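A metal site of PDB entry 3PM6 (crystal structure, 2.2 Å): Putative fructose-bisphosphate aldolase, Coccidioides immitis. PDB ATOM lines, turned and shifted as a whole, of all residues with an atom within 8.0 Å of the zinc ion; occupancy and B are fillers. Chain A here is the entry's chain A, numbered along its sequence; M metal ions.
The nearest printed residue that does not touch the zinc ion is Asp 90 (4.2 Å).
The zinc ion is bound by ND1 of His 227, NE2 of His 91 and NE2 of His 196.
A ring nitrogen (NE2) of His 227 sits close to the side-chain amide nitrogen (ND2) of Asn 249, at 3.4 Å.
NE2 of His 227 is in hydrogen-bond range of OE2 of Glu 148 (2.7 Å).
ND2 of Asn 194 lies within hydrogen-bond range of O of His 227 (2.7 Å).
OD1 of Asp 90 sits close to NE2 of His 91 (3.4 Å).
The backbone NH (N) of His 91 lies within hydrogen-bond range of the side-chain sulfur (SD) of Met 118, at 3.5 Å.
A ring nitrogen (ND1) of His 91 lies within hydrogen-bond range of the side-chain carboxylate of Asp 120.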
ATOM      1  N   CYS A  33      15.615 -27.324  -8.804  1.00  0.00           N
ATOM      2  CA  CYS A  33      15.160 -28.008  -7.613  1.00  0.00           C
ATOM      3  C   CYS A  33      16.184 -28.975  -7.124  1.00  0.00           C
ATOM      4  O   CYS A  33      16.705 -29.807  -7.899  1.00  0.00           O
ATOM      5  CB  CYS A  33      13.874 -28.790  -7.899  1.00  0.00           C
ATOM      6  SG  CYS A  33      12.589 -27.718  -8.473  1.00  0.00           S
ATOM      7  N   LEU A  57      16.215 -24.143  -5.726  1.00  0.00           N
ATOM      8  CA  LEU A  57      14.838 -24.355  -5.294  1.00  0.00           C
ATOM      9  C   LEU A  57      14.732 -25.454  -4.261  1.00  0.00           C
ATOM     10  O   LEU A  57      15.262 -26.535  -4.450  1.00  0.00           O
ATOM     11  CB  LEU A  57      13.927 -24.640  -6.496  1.00  0.00           C
ATOM     12  CG  LEU A  57      13.414 -23.378  -7.208  1.00  0.00           C
ATOM     13  CD1 LEU A  57      14.626 -22.497  -7.709  1.00  0.00           C
ATOM     14  CD2 LEU A  57      12.535 -23.764  -8.389  1.00  0.00           C
ATOM     15  N   PHE A  59      11.802 -27.717  -1.830  1.00  0.00           N
ATOM     16  CA  PHE A  59      10.374 -27.989  -1.645  1.00  0.00           C
ATOM     17  C   PHE A  59      10.023 -27.845  -0.171  1.00  0.00           C
ATOM     18  O   PHE A  59      10.945 -27.773   0.684  1.00  0.00           O
ATOM     19  CB  PHE A  59       9.994 -29.391  -2.145  1.00  0.00           C
ATOM     20  CG  PHE A  59      10.176 -29.576  -3.609  1.00  0.00           C
ATOM     21  CD1 PHE A  59       9.535 -28.729  -4.538  1.00  0.00           C
ATOM     22  CD2 PHE A  59      11.003 -30.563  -4.105  1.00  0.00           C
ATOM     23  CE1 PHE A  59       9.735 -28.880  -5.901  1.00  0.00           C
ATOM     24  CE2 PHE A  59      11.179 -30.715  -5.489  1.00  0.00           C
ATOM     25  CZ  PHE A  59      10.537 -29.878  -6.372  1.00  0.00           C
ATOM     26  N   ASP A  90       9.863 -23.618  -3.777  1.00  0.00           N
ATOM     27  CA  ASP A  90       8.981 -23.971  -4.919  1.00  0.00           C
ATOM     28  C   ASP A  90       7.741 -24.699  -4.403  1.00  0.00           C
ATOM     29  O   ASP A  90       7.808 -25.398  -3.377  1.00  0.00           O
ATOM     30  CB  ASP A  90       9.799 -24.835  -5.898  1.00  0.00           C
ATOM     31  CG  ASP A  90       9.114 -25.082  -7.228  1.00  0.00           C
ATOM     32  OD1 ASP A  90       8.208 -24.316  -7.642  1.00  0.00           O
ATOM     33  OD2 ASP A  90       9.499 -26.104  -7.849  1.00  0.00           O
ATOM     34  N   HIS A  91       6.601 -24.562  -5.098  1.00  0.00           N
ATOM     35  CA  HIS A  91       5.385 -25.352  -4.802  1.00  0.00           C
ATOM     36  C   HIS A  91       5.009 -25.423  -3.319  1.00  0.00           C
ATOM     37  O   HIS A  91       4.728 -26.482  -2.793  1.00  0.00           O
ATOM     38  CB  HIS A  91       5.486 -26.739  -5.447  1.00  0.00           C
ATOM     39  CG  HIS A  91       5.505 -26.626  -6.929  1.00  0.00           C
ATOM     40  ND1 HIS A  91       4.489 -26.013  -7.627  1.00  0.00           N
ATOM     41  CD2 HIS A  91       6.481 -26.882  -7.842  1.00  0.00           C
ATOM     42  CE1 HIS A  91       4.791 -25.957  -8.898  1.00  0.00           C
ATOM     43  NE2 HIS A  91       6.002 -26.477  -9.056  1.00  0.00           N
ATOM     44  N   GLN A  93       2.278 -25.260  -1.143  1.00  0.00           N
ATOM     45  CA  GLN A  93       0.860 -25.379  -1.452  1.00  0.00           C
ATOM     46  C   GLN A  93      -0.032 -25.356  -0.223  1.00  0.00           C
ATOM     47  O   GLN A  93      -1.219 -25.715  -0.293  1.00  0.00           O
ATOM     48  CB  GLN A  93       0.578 -26.628  -2.309  1.00  0.00           C
ATOM     49  CG  GLN A  93       1.372 -26.648  -3.643  1.00  0.00           C
ATOM     50  CD  GLN A  93       1.062 -27.881  -4.489  1.00  0.00           C
ATOM     51  OE1 GLN A  93       0.580 -28.905  -3.975  1.00  0.00           O
ATOM     52  NE2 GLN A  93       1.332 -27.797  -5.788  1.00  0.00           N
ATOM     53  N   MET A 118       7.229 -19.554  -3.817  1.00  0.00           N
ATOM     54  CA  MET A 118       6.127 -19.750  -4.705  1.00  0.00           C
ATOM     55  C   MET A 118       4.858 -19.991  -3.904  1.00  0.00           C
ATOM     56  O   MET A 118       4.714 -21.033  -3.304  1.00  0.00           O
ATOM     57  CB  MET A 118       6.366 -20.893  -5.713  1.00  0.00           C
ATOM     58  CG  MET A 118       5.181 -21.080  -6.637  1.00  0.00           C
ATOM     59  SD  MET A 118       5.278 -22.599  -7.623  1.00  0.00           S
ATOM     60  CE  MET A 118       3.923 -22.222  -8.786  1.00  0.00           C
ATOM     61  N   ASP A 120       1.755 -21.239  -4.178  1.00  0.00           N
ATOM     62  CA  ASP A 120       1.118 -22.091  -5.159  1.00  0.00           C
ATOM     63  C   ASP A 120      -0.220 -22.551  -4.602  1.00  0.00           C
ATOM     64  O   ASP A 120      -0.316 -23.599  -3.956  1.00  0.00           O
ATOM     65  CB  ASP A 120       2.016 -23.322  -5.445  1.00  0.00           C
ATOM     66  CG  ASP A 120       1.413 -24.239  -6.507  1.00  0.00           C
ATOM     67  OD1 ASP A 120       0.319 -23.868  -6.988  1.00  0.00           O
ATOM     68  OD2 ASP A 120       2.026 -25.262  -6.893  1.00  0.00           O
ATOM     69  N   GLU A 148       5.855 -15.796  -6.191  1.00  0.00           N
ATOM     70  CA  GLU A 148       5.447 -16.326  -7.493  1.00  0.00           C
ATOM     71  C   GLU A 148       4.120 -16.961  -7.214  1.00  0.00           C
ATOM     72  O   GLU A 148       3.955 -17.545  -6.152  1.00  0.00           O
ATOM     73  CB  GLU A 148       6.449 -17.374  -7.958  1.00  0.00           C
ATOM     74  CG  GLU A 148       6.078 -18.163  -9.217  1.00  0.00           C
ATOM     75  CD  GLU A 148       7.148 -19.189  -9.588  1.00  0.00           C
ATOM     76  OE1 GLU A 148       8.357 -18.886  -9.457  1.00  0.00           O
ATOM     77  OE2 GLU A 148       6.770 -20.310  -9.993  1.00  0.00           O
ATOM     78  N   GLU A 150       0.551 -19.054  -9.291  1.00  0.00           N
ATOM     79  CA  GLU A 150       0.104 -19.818 -10.473  1.00  0.00           C
ATOM     80  C   GLU A 150      -1.335 -19.489 -10.858  1.00  0.00           C
ATOM     81  O   GLU A 150      -2.305 -20.016 -10.265  1.00  0.00           O
ATOM     82  CB  GLU A 150       0.225 -21.312 -10.189  1.00  0.00           C
ATOM     83  CG  GLU A 150      -0.102 -22.202 -11.388  1.00  0.00           C
ATOM     84  CD  GLU A 150       0.274 -23.670 -11.115  1.00  0.00           C
ATOM     85  OE1 GLU A 150       1.390 -23.923 -10.630  1.00  0.00           O
ATOM     86  OE2 GLU A 150      -0.515 -24.551 -11.420  1.00  0.00           O
ATOM     87  N   ILE A 154      -1.524 -26.332 -13.394  1.00  0.00           N
ATOM     88  CA  ILE A 154      -0.669 -27.314 -14.010  1.00  0.00           C
ATOM     89  C   ILE A 154      -0.979 -28.679 -13.391  1.00  0.00           C
ATOM     90  O   ILE A 154      -1.099 -28.822 -12.157  1.00  0.00           O
ATOM     91  CB  ILE A 154       0.846 -26.902 -13.869  1.00  0.00           C
ATOM     92  CG1 ILE A 154       1.092 -25.539 -14.544  1.00  0.00           C
ATOM     93  CG2 ILE A 154       1.755 -27.946 -14.521  1.00  0.00           C
ATOM     94  CD1 ILE A 154       2.406 -24.849 -14.161  1.00  0.00           C
ATOM     95  N   GLU A 158       5.338 -34.491  -8.726  1.00  0.00           N
ATOM     96  CA  GLU A 158       6.758 -34.885  -8.684  1.00  0.00           C
ATOM     97  C   GLU A 158       7.073 -35.271  -7.226  1.00  0.00           C
ATOM     98  O   GLU A 158       6.243 -35.073  -6.355  1.00  0.00           O
ATOM     99  CB  GLU A 158       7.669 -33.746  -9.238  1.00  0.00           C
ATOM    100  CG  GLU A 158       7.287 -33.378 -10.719  1.00  0.00           C
ATOM    101  CD  GLU A 158       8.139 -32.276 -11.351  1.00  0.00           C
ATOM    102  OE1 GLU A 158       8.940 -31.697 -10.618  1.00  0.00           O
ATOM    103  OE2 GLU A 158       8.000 -31.984 -12.589  1.00  0.00           O
ATOM    104  N   VAL A 161       6.155 -32.644  -4.796  1.00  0.00           N
ATOM    105  CA  VAL A 161       5.067 -31.791  -5.360  1.00  0.00           C
ATOM    106  C   VAL A 161       3.803 -32.643  -5.463  1.00  0.00           C
ATOM    107  O   VAL A 161       3.808 -33.655  -6.160  1.00  0.00           O
ATOM    108  CB  VAL A 161       5.490 -31.187  -6.755  1.00  0.00           C
ATOM    109  CG1 VAL A 161       4.365 -30.294  -7.386  1.00  0.00           C
ATOM    110  CG2 VAL A 161       6.787 -30.372  -6.618  1.00  0.00           C
ATOM    111  N   ALA A 189       3.489 -18.184 -12.905  1.00  0.00           N
ATOM    112  CA  ALA A 189       3.774 -19.492 -13.493  1.00  0.00           C
ATOM    113  C   ALA A 189       2.560 -19.871 -14.323  1.00  0.00           C
ATOM    114  O   ALA A 189       1.563 -20.355 -13.775  1.00  0.00           O
ATOM    115  CB  ALA A 189       3.976 -20.526 -12.385  1.00  0.00           C
ATOM    116  N   ASN A 194       2.064 -27.070 -20.500  1.00  0.00           N
ATOM    117  CA  ASN A 194       3.080 -27.727 -19.696  1.00  0.00           C
ATOM    118  C   ASN A 194       2.448 -28.592 -18.579  1.00  0.00           C
ATOM    119  O   ASN A 194       1.273 -28.396 -18.203  1.00  0.00           O
ATOM    120  CB  ASN A 194       4.098 -26.735 -19.137  1.00  0.00           C
ATOM    121  CG  ASN A 194       3.466 -25.559 -18.428  1.00  0.00           C
ATOM    122  OD1 ASN A 194       2.312 -25.187 -18.691  1.00  0.00           O
ATOM    123  ND2 ASN A 194       4.221 -24.935 -17.545  1.00  0.00           N
ATOM    124  N   VAL A 195       3.212 -29.581 -18.113  1.00  0.00           N
ATOM    125  CA  VAL A 195       2.736 -30.624 -17.199  1.00  0.00           C
ATOM    126  C   VAL A 195       3.931 -30.939 -16.296  1.00  0.00           C
ATOM    127  O   VAL A 195       5.101 -30.974 -16.753  1.00  0.00           O
ATOM    128  CB  VAL A 195       2.305 -31.920 -17.996  1.00  0.00           C
ATOM    129  CG1 VAL A 195       2.313 -33.134 -17.148  1.00  0.00           C
ATOM    130  CG2 VAL A 195       0.943 -31.799 -18.584  1.00  0.00           C
ATOM    131  N   HIS A 196       3.667 -31.124 -15.015  1.00  0.00           N
ATOM    132  CA  HIS A 196       4.672 -31.697 -14.118  1.00  0.00           C
ATOM    133  C   HIS A 196       4.771 -33.190 -14.370  1.00  0.00           C
ATOM    134  O   HIS A 196       3.768 -33.852 -14.601  1.00  0.00           O
ATOM    135  CB  HIS A 196       4.283 -31.450 -12.657  1.00  0.00           C
ATOM    136  CG  HIS A 196       4.463 -30.037 -12.214  1.00  0.00           C
ATOM    137  ND1 HIS A 196       3.451 -29.298 -11.623  1.00  0.00           N
ATOM    138  CD2 HIS A 196       5.535 -29.206 -12.288  1.00  0.00           C
ATOM    139  CE1 HIS A 196       3.908 -28.095 -11.330  1.00  0.00           C
ATOM    140  NE2 HIS A 196       5.163 -28.010 -11.725  1.00  0.00           N
ATOM    141  N   GLY A 197       5.993 -33.725 -14.268  1.00  0.00           N
ATOM    142  CA  GLY A 197       6.255 -35.155 -14.533  1.00  0.00           C
ATOM    143  C   GLY A 197       6.253 -35.561 -15.999  1.00  0.00           C
ATOM    144  O   GLY A 197       6.451 -34.750 -16.882  1.00  0.00           O
ATOM    145  N   VAL A 225       7.355 -17.556 -15.466  1.00  0.00           N
ATOM    146  CA  VAL A 225       8.075 -18.694 -14.912  1.00  0.00           C
ATOM    147  C   VAL A 225       7.582 -19.951 -15.570  1.00  0.00           C
ATOM    148  O   VAL A 225       6.375 -20.245 -15.560  1.00  0.00           O
ATOM    149  CB  VAL A 225       7.908 -18.774 -13.351  1.00  0.00           C
ATOM    150  CG1 VAL A 225       8.790 -19.877 -12.754  1.00  0.00           C
ATOM    151  CG2 VAL A 225       8.304 -17.436 -12.719  1.00  0.00           C
ATOM    152  N   LEU A 226       8.541 -20.701 -16.132  1.00  0.00           N
ATOM    153  CA  LEU A 226       8.283 -21.937 -16.844  1.00  0.00           C
ATOM    154  C   LEU A 226       8.418 -23.130 -15.892  1.00  0.00           C
ATOM    155  O   LEU A 226       9.474 -23.377 -15.305  1.00  0.00           O
ATOM    156  CB  LEU A 226       9.261 -22.094 -18.016  1.00  0.00           C
ATOM    157  CG  LEU A 226       9.096 -23.343 -18.911  1.00  0.00           C
ATOM    158  CD1 LEU A 226       7.692 -23.492 -19.465  1.00  0.00           C
ATOM    159  CD2 LEU A 226      10.080 -23.324 -20.077  1.00  0.00           C
ATOM    160  N   HIS A 227       7.327 -23.878 -15.788  1.00  0.00           N
ATOM    161  CA  HIS A 227       7.275 -25.151 -15.038  1.00  0.00           C
ATOM    162  C   HIS A 227       7.087 -26.319 -15.992  1.00  0.00           C
ATOM    163  O   HIS A 227       6.592 -26.112 -17.126  1.00  0.00           O
ATOM    164  CB  HIS A 227       6.049 -25.128 -14.097  1.00  0.00           C
ATOM    165  CG  HIS A 227       6.242 -24.258 -12.896  1.00  0.00           C
ATOM    166  ND1 HIS A 227       6.476 -24.777 -11.647  1.00  0.00           N
ATOM    167  CD2 HIS A 227       6.272 -22.909 -12.757  1.00  0.00           C
ATOM    168  CE1 HIS A 227       6.648 -23.784 -10.781  1.00  0.00           C
ATOM    169  NE2 HIS A 227       6.522 -22.641 -11.430  1.00  0.00           N
ATOM    170  N   GLY A 228       7.434 -27.525 -15.529  1.00  0.00           N
ATOM    171  CA  GLY A 228       7.353 -28.737 -16.308  1.00  0.00           C
ATOM    172  C   GLY A 228       8.307 -28.839 -17.500  1.00  0.00           C
ATOM    173  O   GLY A 228       8.006 -29.490 -18.518  1.00  0.00           O
ATOM    174  N   ALA A 229       9.473 -28.242 -17.348  1.00  0.00           N
ATOM    175  CA  ALA A 229      10.417 -28.049 -18.419  1.00  0.00           C
ATOM    176  C   ALA A 229      11.472 -29.172 -18.571  1.00  0.00           C
ATOM    177  O   ALA A 229      12.280 -29.135 -19.491  1.00  0.00           O
ATOM    178  CB  ALA A 229      11.093 -26.674 -18.239  1.00  0.00           C
ATOM    179  N   LYS A 247      12.397 -17.226 -16.033  1.00  0.00           N
ATOM    180  CA  LYS A 247      12.822 -18.180 -15.019  1.00  0.00           C
ATOM    181  C   LYS A 247      12.378 -19.538 -15.512  1.00  0.00           C
ATOM    182  O   LYS A 247      11.182 -19.744 -15.822  1.00  0.00           O
ATOM    183  CB  LYS A 247      12.184 -17.851 -13.665  1.00  0.00           C
ATOM    184  CG  LYS A 247      12.527 -18.821 -12.502  1.00  0.00           C
ATOM    185  CD  LYS A 247      11.924 -18.281 -11.188  1.00  0.00           C
ATOM    186  CE  LYS A 247      11.990 -19.247 -10.021  1.00  0.00           C
ATOM    187  NZ  LYS A 247      10.797 -20.139  -9.956  1.00  0.00           N
ATOM    188  N   ASN A 249      12.330 -23.515 -14.375  1.00  0.00           N
ATOM    189  CA  ASN A 249      12.411 -24.509 -13.324  1.00  0.00           C
ATOM    190  C   ASN A 249      12.759 -25.879 -13.867  1.00  0.00           C
ATOM    191  O   ASN A 249      12.140 -26.350 -14.844  1.00  0.00           O
ATOM    192  CB  ASN A 249      11.056 -24.649 -12.577  1.00  0.00           C
ATOM    193  CG  ASN A 249      10.727 -23.433 -11.713  1.00  0.00           C
ATOM    194  OD1 ASN A 249      11.387 -22.388 -11.819  1.00  0.00           O
ATOM    195  ND2 ASN A 249       9.728 -23.553 -10.856  1.00  0.00           N
ATOM    196  N   VAL A 250      13.638 -26.553 -13.136  1.00  0.00           N
ATOM    197  CA  VAL A 250      14.132 -27.850 -13.526  1.00  0.00           C
ATOM    198  C   VAL A 250      14.167 -28.735 -12.311  1.00  0.00           C
ATOM    199  O   VAL A 250      14.486 -28.284 -11.223  1.00  0.00           O
ATOM    200  CB  VAL A 250      15.577 -27.722 -14.056  1.00  0.00           C
ATOM    201  CG1 VAL A 250      16.100 -29.058 -14.501  1.00  0.00           C
ATOM    202  CG2 VAL A 250      15.626 -26.741 -15.212  1.00  0.00           C
ATOM    203  N   ASN A 251      13.852 -30.007 -12.500  1.00  0.00           N
ATOM    204  CA  ASN A 251      13.965 -30.965 -11.408  1.00  0.00           C
ATOM    205  C   ASN A 251      14.638 -32.290 -11.852  1.00  0.00           C
ATOM    206  O   ASN A 251      15.857 -32.459 -11.685  1.00  0.00           O
ATOM    207  CB  ASN A 251      12.589 -31.204 -10.734  1.00  0.00           C
ATOM    208  CG  ASN A 251      12.683 -32.145  -9.567  1.00  0.00           C
ATOM    209  OD1 ASN A 251      13.784 -32.564  -9.215  1.00  0.00           O
ATOM    210  ND2 ASN A 251      11.544 -32.510  -8.948  1.00  0.00           N
HETATM  211 ZN    ZN M   1       6.798 -26.744 -10.984  1.00  0.00          ZN
